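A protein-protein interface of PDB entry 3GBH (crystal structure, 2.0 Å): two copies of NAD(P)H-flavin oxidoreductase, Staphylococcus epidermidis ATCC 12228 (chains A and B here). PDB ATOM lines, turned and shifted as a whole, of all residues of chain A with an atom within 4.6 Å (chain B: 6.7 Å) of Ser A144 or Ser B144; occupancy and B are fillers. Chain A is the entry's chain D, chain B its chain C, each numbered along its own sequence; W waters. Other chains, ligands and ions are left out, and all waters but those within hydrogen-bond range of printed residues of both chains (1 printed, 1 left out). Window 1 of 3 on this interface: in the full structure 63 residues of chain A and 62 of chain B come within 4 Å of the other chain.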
ATOM      1  N   ASN A 140      -2.298   1.887  -5.581  1.00  0.00           N
ATOM      2  CA  ASN A 140      -3.740   1.966  -5.843  1.00  0.00           C
ATOM      3  C   ASN A 140      -4.326   0.602  -6.244  1.00  0.00           C
ATOM      4  O   ASN A 140      -5.364   0.174  -5.734  1.00  0.00           O
ATOM      5  CB  ASN A 140      -4.053   2.958  -6.969  1.00  0.00           C
ATOM      6  CG  ASN A 140      -4.072   4.405  -6.524  1.00  0.00           C
ATOM      7  OD1 ASN A 140      -4.298   4.719  -5.366  1.00  0.00           O
ATOM      8  ND2 ASN A 140      -3.911   5.307  -7.489  1.00  0.00           N
ATOM      9  N   ILE A 141      -3.652  -0.064  -7.169  1.00  0.00           N
ATOM     10  CA  ILE A 141      -4.037  -1.393  -7.606  1.00  0.00           C
ATOM     11  C   ILE A 141      -4.000  -2.421  -6.473  1.00  0.00           C
ATOM     12  O   ILE A 141      -5.014  -3.086  -6.213  1.00  0.00           O
ATOM     13  CB  ILE A 141      -3.170  -1.844  -8.828  1.00  0.00           C
ATOM     14  CG1 ILE A 141      -3.537  -0.981 -10.029  1.00  0.00           C
ATOM     15  CG2 ILE A 141      -3.360  -3.348  -9.122  1.00  0.00           C
ATOM     16  CD1 ILE A 141      -2.595  -1.082 -11.189  1.00  0.00           C
ATOM     17  N   ASP A 142      -2.866  -2.560  -5.786  1.00  0.00           N
ATOM     18  CA  ASP A 142      -2.743  -3.534  -4.686  1.00  0.00           C
ATOM     19  C   ASP A 142      -3.808  -3.272  -3.606  1.00  0.00           C
ATOM     20  O   ASP A 142      -4.515  -4.186  -3.164  1.00  0.00           O
ATOM     21  CB  ASP A 142      -1.368  -3.442  -3.999  1.00  0.00           C
ATOM     22  CG  ASP A 142      -0.204  -3.939  -4.844  1.00  0.00           C
ATOM     23  OD1 ASP A 142      -0.384  -4.714  -5.828  1.00  0.00           O
ATOM     24  OD2 ASP A 142       0.936  -3.561  -4.473  1.00  0.00           O
ATOM     25  N   SER A 143      -3.904  -2.018  -3.164  1.00  0.00           N
ATOM     26  CA  SER A 143      -4.824  -1.674  -2.058  1.00  0.00           C
ATOM     27  C   SER A 143      -6.301  -1.954  -2.401  1.00  0.00           C
ATOM     28  O   SER A 143      -7.096  -2.339  -1.526  1.00  0.00           O
ATOM     29  CB  SER A 143      -4.600  -0.232  -1.664  1.00  0.00           C
ATOM     30  OG  SER A 143      -3.258  -0.052  -1.177  1.00  0.00           O
ATOM     31  N   SER A 144      -6.643  -1.814  -3.681  1.00  0.00           N
ATOM     32  CA  SER A 144      -8.004  -2.047  -4.202  1.00  0.00           C
ATOM     33  C   SER A 144      -8.302  -3.529  -4.246  1.00  0.00           C
ATOM     34  O   SER A 144      -9.419  -3.967  -3.939  1.00  0.00           O
ATOM     35  CB  SER A 144      -8.181  -1.438  -5.579  1.00  0.00           C
ATOM     36  OG  SER A 144      -8.064  -0.019  -5.531  1.00  0.00           O
ATOM     37  N   LEU A 145      -7.297  -4.312  -4.595  1.00  0.00           N
ATOM     38  CA  LEU A 145      -7.442  -5.761  -4.548  1.00  0.00           C
ATOM     39  C   LEU A 145      -7.795  -6.223  -3.138  1.00  0.00           C
ATOM     40  O   LEU A 145      -8.752  -6.989  -2.949  1.00  0.00           O
ATOM     41  CB  LEU A 145      -6.145  -6.444  -5.017  1.00  0.00           C
ATOM     42  CG  LEU A 145      -5.776  -6.295  -6.491  1.00  0.00           C
ATOM     43  CD1 LEU A 145      -4.398  -6.935  -6.720  1.00  0.00           C
ATOM     44  CD2 LEU A 145      -6.828  -6.920  -7.421  1.00  0.00           C
ATOM     45  N   MET A 146      -7.021  -5.758  -2.156  1.00  0.00           N
ATOM     46  CA  MET A 146      -7.304  -6.007  -0.739  1.00  0.00           C
ATOM     47  C   MET A 146      -8.698  -5.503  -0.359  1.00  0.00           C
ATOM     48  O   MET A 146      -9.459  -6.218   0.332  1.00  0.00           O
ATOM     49  CB  MET A 146      -6.247  -5.333   0.151  1.00  0.00           C
ATOM     50  CG  MET A 146      -6.305  -5.687   1.586  1.00  0.00           C
ATOM     51  SD  MET A 146      -7.528  -4.540   2.573  1.00  0.00           S
ATOM     52  CE  MET A 146      -6.467  -2.893   2.541  1.00  0.00           C
ATOM     53  N   ALA A 147      -9.032  -4.279  -0.778  1.00  0.00           N
ATOM     54  CA  ALA A 147     -10.346  -3.693  -0.459  1.00  0.00           C
ATOM     55  C   ALA A 147     -11.500  -4.578  -0.874  1.00  0.00           C
ATOM     56  O   ALA A 147     -12.450  -4.734  -0.102  1.00  0.00           O
ATOM     57  CB  ALA A 147     -10.515  -2.284  -1.082  1.00  0.00           C
ATOM     58  N   MET A 148     -11.453  -5.119  -2.093  1.00  0.00           N
ATOM     59  CA  MET A 148     -12.527  -5.988  -2.581  1.00  0.00           C
ATOM     60  C   MET A 148     -12.657  -7.246  -1.719  1.00  0.00           C
ATOM     61  O   MET A 148     -13.746  -7.615  -1.277  1.00  0.00           O
ATOM     62  CB  MET A 148     -12.291  -6.386  -4.039  1.00  0.00           C
ATOM     63  CG  MET A 148     -13.411  -7.244  -4.646  1.00  0.00           C
ATOM     64  SD  MET A 148     -14.961  -6.100  -5.048  1.00  0.00           S
ATOM     65  CE  MET A 148     -16.178  -6.695  -3.612  1.00  0.00           C
ATOM     66  N   VAL A 186      -6.366   5.847  -0.994  1.00  0.00           N
ATOM     67  CA  VAL A 186      -6.848   5.114  -2.159  1.00  0.00           C
ATOM     68  C   VAL A 186      -8.381   5.075  -2.191  1.00  0.00           C
ATOM     69  O   VAL A 186      -9.003   5.558  -3.131  1.00  0.00           O
ATOM     70  CB  VAL A 186      -6.302   3.657  -2.128  1.00  0.00           C
ATOM     71  CG1 VAL A 186      -6.826   2.860  -3.305  1.00  0.00           C
ATOM     72  CG2 VAL A 186      -4.767   3.697  -2.062  1.00  0.00           C
ATOM     73  N   TRP B  54     -14.043  -0.942 -16.644  1.00  0.00           N
ATOM     74  CA  TRP B  54     -13.255  -2.108 -16.976  1.00  0.00           C
ATOM     75  C   TRP B  54     -13.567  -2.690 -18.366  1.00  0.00           C
ATOM     76  O   TRP B  54     -14.736  -2.787 -18.757  1.00  0.00           O
ATOM     77  CB  TRP B  54     -13.424  -3.183 -15.899  1.00  0.00           C
ATOM     78  CG  TRP B  54     -14.800  -3.449 -15.436  1.00  0.00           C
ATOM     79  CD1 TRP B  54     -15.809  -4.001 -16.141  1.00  0.00           C
ATOM     80  CD2 TRP B  54     -15.333  -3.141 -14.144  1.00  0.00           C
ATOM     81  NE1 TRP B  54     -16.940  -4.079 -15.374  1.00  0.00           N
ATOM     82  CE2 TRP B  54     -16.665  -3.570 -14.131  1.00  0.00           C
ATOM     83  CE3 TRP B  54     -14.800  -2.568 -12.992  1.00  0.00           C
ATOM     84  CZ2 TRP B  54     -17.466  -3.456 -13.016  1.00  0.00           C
ATOM     85  CZ3 TRP B  54     -15.593  -2.464 -11.881  1.00  0.00           C
ATOM     86  CH2 TRP B  54     -16.912  -2.890 -11.902  1.00  0.00           C
ATOM     87  N   ILE B  88      -6.677  -6.493 -18.572  1.00  0.00           N
ATOM     88  CA  ILE B  88      -7.736  -5.588 -18.115  1.00  0.00           C
ATOM     89  C   ILE B  88      -7.306  -4.148 -18.346  1.00  0.00           C
ATOM     90  O   ILE B  88      -6.271  -3.720 -17.832  1.00  0.00           O
ATOM     91  CB  ILE B  88      -8.054  -5.799 -16.634  1.00  0.00           C
ATOM     92  CG1 ILE B  88      -8.396  -7.283 -16.380  1.00  0.00           C
ATOM     93  CG2 ILE B  88      -9.210  -4.850 -16.179  1.00  0.00           C
ATOM     94  CD1 ILE B  88      -8.551  -7.620 -14.938  1.00  0.00           C
ATOM     95  N   ASP B 137      -6.538   7.221 -11.991  1.00  0.00           N
ATOM     96  CA  ASP B 137      -6.705   6.691 -10.620  1.00  0.00           C
ATOM     97  C   ASP B 137      -8.054   5.991 -10.475  1.00  0.00           C
ATOM     98  O   ASP B 137      -8.120   4.873  -9.966  1.00  0.00           O
ATOM     99  CB  ASP B 137      -6.580   7.804  -9.585  1.00  0.00           C
ATOM    100  CG  ASP B 137      -5.173   8.360  -9.458  1.00  0.00           C
ATOM    101  OD1 ASP B 137      -4.193   7.735  -9.923  1.00  0.00           O
ATOM    102  OD2 ASP B 137      -5.055   9.464  -8.867  1.00  0.00           O
ATOM    103  N   VAL B 139     -10.056   4.609 -12.775  1.00  0.00           N
ATOM    104  CA  VAL B 139     -10.210   3.354 -13.495  1.00  0.00           C
ATOM    105  C   VAL B 139      -9.261   2.266 -12.980  1.00  0.00           C
ATOM    106  O   VAL B 139      -9.612   1.098 -13.083  1.00  0.00           O
ATOM    107  CB  VAL B 139     -10.105   3.492 -15.030  1.00  0.00           C
ATOM    108  CG1 VAL B 139     -11.140   4.521 -15.570  1.00  0.00           C
ATOM    109  CG2 VAL B 139      -8.664   3.810 -15.510  1.00  0.00           C
ATOM    110  N   ASN B 140      -8.085   2.621 -12.437  1.00  0.00           N
ATOM    111  CA  ASN B 140      -7.209   1.593 -11.827  1.00  0.00           C
ATOM    112  C   ASN B 140      -7.899   0.957 -10.625  1.00  0.00           C
ATOM    113  O   ASN B 140      -7.859  -0.257 -10.413  1.00  0.00           O
ATOM    114  CB  ASN B 140      -5.857   2.192 -11.398  1.00  0.00           C
ATOM    115  CG  ASN B 140      -4.887   2.389 -12.569  1.00  0.00           C
ATOM    116  OD1 ASN B 140      -5.034   1.767 -13.607  1.00  0.00           O
ATOM    117  ND2 ASN B 140      -3.917   3.278 -12.401  1.00  0.00           N
ATOM    118  N   ILE B 141      -8.512   1.797  -9.804  1.00  0.00           N
ATOM    119  CA  ILE B 141      -9.158   1.334  -8.593  1.00  0.00           C
ATOM    120  C   ILE B 141     -10.358   0.455  -8.946  1.00  0.00           C
ATOM    121  O   ILE B 141     -10.460  -0.673  -8.455  1.00  0.00           O
ATOM    122  CB  ILE B 141      -9.545   2.531  -7.685  1.00  0.00           C
ATOM    123  CG1 ILE B 141      -8.270   3.143  -7.095  1.00  0.00           C
ATOM    124  CG2 ILE B 141     -10.499   2.114  -6.536  1.00  0.00           C
ATOM    125  CD1 ILE B 141      -8.471   4.568  -6.457  1.00  0.00           C
ATOM    126  N   ASP B 142     -11.242   0.936  -9.825  1.00  0.00           N
ATOM    127  CA  ASP B 142     -12.437   0.191 -10.161  1.00  0.00           C
ATOM    128  C   ASP B 142     -12.061  -1.156 -10.771  1.00  0.00           C
ATOM    129  O   ASP B 142     -12.590  -2.175 -10.364  1.00  0.00           O
ATOM    130  CB  ASP B 142     -13.333   0.945 -11.156  1.00  0.00           C
ATOM    131  CG  ASP B 142     -14.046   2.141 -10.553  1.00  0.00           C
ATOM    132  OD1 ASP B 142     -14.190   2.244  -9.305  1.00  0.00           O
ATOM    133  OD2 ASP B 142     -14.499   2.991 -11.365  1.00  0.00           O
ATOM    134  N   SER B 143     -11.135  -1.135 -11.733  1.00  0.00           N
ATOM    135  CA  SER B 143     -10.768  -2.338 -12.486  1.00  0.00           C
ATOM    136  C   SER B 143     -10.110  -3.393 -11.592  1.00  0.00           C
ATOM    137  O   SER B 143     -10.237  -4.596 -11.833  1.00  0.00           O
ATOM    138  CB  SER B 143      -9.833  -1.971 -13.628  1.00  0.00           C
ATOM    139  OG  SER B 143     -10.497  -1.117 -14.560  1.00  0.00           O
ATOM    140  N   SER B 144      -9.398  -2.930 -10.569  1.00  0.00           N
ATOM    141  CA  SER B 144      -8.748  -3.810  -9.585  1.00  0.00           C
ATOM    142  C   SER B 144      -9.757  -4.463  -8.651  1.00  0.00           C
ATOM    143  O   SER B 144      -9.626  -5.658  -8.300  1.00  0.00           O
ATOM    144  CB  SER B 144      -7.714  -3.020  -8.780  1.00  0.00           C
ATOM    145  OG  SER B 144      -6.671  -2.600  -9.631  1.00  0.00           O
ATOM    146  N   LEU B 145     -10.767  -3.692  -8.231  1.00  0.00           N
ATOM    147  CA  LEU B 145     -11.877  -4.271  -7.481  1.00  0.00           C
ATOM    148  C   LEU B 145     -12.468  -5.467  -8.243  1.00  0.00           C
ATOM    149  O   LEU B 145     -12.624  -6.571  -7.701  1.00  0.00           O
ATOM    150  CB  LEU B 145     -12.955  -3.206  -7.202  1.00  0.00           C
ATOM    151  CG  LEU B 145     -12.545  -2.059  -6.268  1.00  0.00           C
ATOM    152  CD1 LEU B 145     -13.664  -1.018  -6.142  1.00  0.00           C
ATOM    153  CD2 LEU B 145     -12.170  -2.609  -4.876  1.00  0.00           C
ATOM    154  N   MET B 146     -12.810  -5.237  -9.502  1.00  0.00           N
ATOM    155  CA  MET B 146     -13.328  -6.282 -10.393  1.00  0.00           C
ATOM    156  C   MET B 146     -12.379  -7.467 -10.520  1.00  0.00           C
ATOM    157  O   MET B 146     -12.801  -8.619 -10.401  1.00  0.00           O
ATOM    158  CB  MET B 146     -13.624  -5.712 -11.769  1.00  0.00           C
ATOM    159  CG  MET B 146     -14.333  -6.661 -12.692  1.00  0.00           C
ATOM    160  SD  MET B 146     -13.158  -7.846 -13.648  1.00  0.00           S
ATOM    161  CE  MET B 146     -12.360  -6.369 -14.687  1.00  0.00           C
ATOM    162  N   ALA B 147     -11.092  -7.181 -10.724  1.00  0.00           N
ATOM    163  CA  ALA B 147     -10.060  -8.201 -10.855  1.00  0.00           C
ATOM    164  C   ALA B 147      -9.985  -9.160  -9.689  1.00  0.00           C
ATOM    165  O   ALA B 147      -9.887 -10.375  -9.893  1.00  0.00           O
ATOM    166  CB  ALA B 147      -8.655  -7.559 -11.132  1.00  0.00           C
ATOM    167  N   MET B 148     -10.044  -8.635  -8.466  1.00  0.00           N
ATOM    168  CA  MET B 148     -10.024  -9.466  -7.295  1.00  0.00           C
ATOM    169  C   MET B 148     -11.224 -10.399  -7.272  1.00  0.00           C
ATOM    170  O   MET B 148     -11.079 -11.595  -7.032  1.00  0.00           O
ATOM    171  CB  MET B 148      -9.982  -8.597  -6.013  1.00  0.00           C
ATOM    172  CG  MET B 148      -9.855  -9.401  -4.754  1.00  0.00           C
ATOM    173  SD  MET B 148      -8.079 -10.062  -4.473  1.00  0.00           S
ATOM    174  CE  MET B 148      -8.267 -11.990  -4.791  1.00  0.00           C
ATOM    175  N   GLN B 149     -12.422  -9.871  -7.530  1.00  0.00           N
ATOM    176  CA  GLN B 149     -13.609 -10.729  -7.573  1.00  0.00           C
ATOM    177  C   GLN B 149     -13.486 -11.799  -8.684  1.00  0.00           C
ATOM    178  O   GLN B 149     -13.963 -12.929  -8.531  1.00  0.00           O
ATOM    179  CB  GLN B 149     -14.887  -9.865  -7.638  1.00  0.00           C
ATOM    180  CG  GLN B 149     -16.210 -10.623  -7.472  1.00  0.00           C
ATOM    181  CD  GLN B 149     -17.341  -9.736  -6.994  1.00  0.00           C
ATOM    182  OE1 GLN B 149     -17.296  -9.233  -5.885  1.00  0.00           O
ATOM    183  NE2 GLN B 149     -18.405  -9.604  -7.807  1.00  0.00           N
ATOM    184  N   MET B 151     -10.606 -13.230  -9.715  1.00  0.00           N
ATOM    185  CA  MET B 151      -9.680 -14.264  -9.245  1.00  0.00           C
ATOM    186  C   MET B 151     -10.357 -15.172  -8.244  1.00  0.00           C
ATOM    187  O   MET B 151     -10.153 -16.388  -8.250  1.00  0.00           O
ATOM    188  CB  MET B 151      -8.423 -13.636  -8.668  1.00  0.00           C
ATOM    189  CG  MET B 151      -7.600 -13.004  -9.727  1.00  0.00           C
ATOM    190  SD  MET B 151      -5.885 -12.407  -9.060  1.00  0.00           S
ATOM    191  CE  MET B 151      -6.419 -10.706  -8.271  1.00  0.00           C
ATOM    192  N   VAL B 186      -4.371  -1.899 -16.835  1.00  0.00           N
ATOM    193  CA  VAL B 186      -4.376  -1.829 -15.402  1.00  0.00           C
ATOM    194  C   VAL B 186      -3.542  -2.978 -14.836  1.00  0.00           C
ATOM    195  O   VAL B 186      -2.561  -2.757 -14.142  1.00  0.00           O
ATOM    196  CB  VAL B 186      -5.814  -1.885 -14.846  1.00  0.00           C
ATOM    197  CG1 VAL B 186      -5.740  -1.933 -13.331  1.00  0.00           C
ATOM    198  CG2 VAL B 186      -6.643  -0.695 -15.371  1.00  0.00           C
ATOM    199  N   LEU B 187      -3.949  -4.203 -15.152  1.00  0.00           N
ATOM    200  CA  LEU B 187      -3.198  -5.405 -14.818  1.00  0.00           C
ATOM    201  C   LEU B 187      -3.649  -6.569 -15.734  1.00  0.00           C
ATOM    202  O   LEU B 187      -4.672  -6.494 -16.420  1.00  0.00           O
ATOM    203  CB  LEU B 187      -3.369  -5.785 -13.336  1.00  0.00           C
ATOM    204  CG  LEU B 187      -4.643  -6.533 -12.930  1.00  0.00           C
ATOM    205  CD1 LEU B 187      -4.486  -7.263 -11.557  1.00  0.00           C
ATOM    206  CD2 LEU B 187      -5.831  -5.559 -12.889  1.00  0.00           C
HETATM  207  O   HOH W   1      -3.448   5.170 -10.280  1.00  0.00           O
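Ile A141 touches Ser B144, and with the chains exchanged Ser A144 touches Ile B141. Ile A141 touches Val B186, and with the chains exchanged Val A186 touches Ile B141. Leu A145 touches Met B148, and with the chains exchanged Met A148 touches Leu B145. Met B148 touches its own counterpart, Met A148. 10 positions are printed for both chains. Of the 13 pairs that touch across the chains among the printed residues, 10 have their exchanged pair printed and touching as well.
Among the printed residues, merely in contact across the chains: Ile A141 with Ser B144, Ile A141 with Val B186, Ser A144 with Ile B141, Ser A144 with Ser B144, Ser A144 with Leu B145, Leu A145 with Ser B144, Leu A145 with Met B151, Met A148 with Met B148, Met A148 with Gln B149 and Val A186 with Ile B141.
OG of Ser B144 lies within hydrogen-bond range of O of Asn B140, 2.7 Å away. The backbone carbonyl oxygen (O) of Asn A140 sits at hydrogen-bond distance from the side-chain hydroxyl (OG) of Ser A144, 2.7 Å away. N of Val B186 is in hydrogen-bond range of O of Ile B88, at 2.8 Å.
Water W1 lies within hydrogen-bond range of OD1 of Asp B137 (2.7 Å), ND2 of Asn A140 (2.8 Å) and ND2 of Asn B140 (2.9 Å).
Hydrophobic or aromatic side chains of chain A within 4 Å of the printed part of chain B: Ile A141, Leu A145, Met A148 and Val A186. Hydrophobic or aromatic side chains of chain B within 4 Å of the printed part of chain A: Ile B141, Leu B145, Met B148, Met B151 and Val B186. Among the printed residues, 13 pairs touch across the chains. Among the printed residues, no Asp or Glu carboxylate lies within 4 Å of a Lys or Arg side-chain nitrogen of the other chain.
Of the printed residues of chain B, Asn A140 touches Asp B137. Ser A144 touches just these residues of chain B: Ile B141 (3.4 Å), Ser B144 (3.6 Å) and Leu B145 (3.2 Å). Of the printed residues of chain B, Met A148 touches Leu B145, Met B148 and Gln B149. Printed residues of chain A within 4 Å of Asp B137: Asn A140 (3.4 Å). Val B139 touches none of the printed residues of chain A. Of chain A, only Ile A141 (3.4 Å), Ser A144 (3.6 Å) and Leu A145 (3.2 Å) come within 4 Å of Ser B144. Of the printed residues of chain A, Leu B145 touches Ser A144 (3.2 Å) and Met A148 (3.2 Å).
The side-chain sulfur (SD) of Met A148 sits close to the backbone carbonyl oxygen (O) of Leu B145 (3.6 Å). The side-chain amide nitrogen (ND2) of Asn A140 sits at hydrogen-bond distance from the side-chain carboxylate (OD1) of Asp B137 (3.4 Å). The backbone carbonyl oxygen (O) of Leu A145 lies close to the side-chain sulfur (SD) of Met B148 (3.5 Å).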
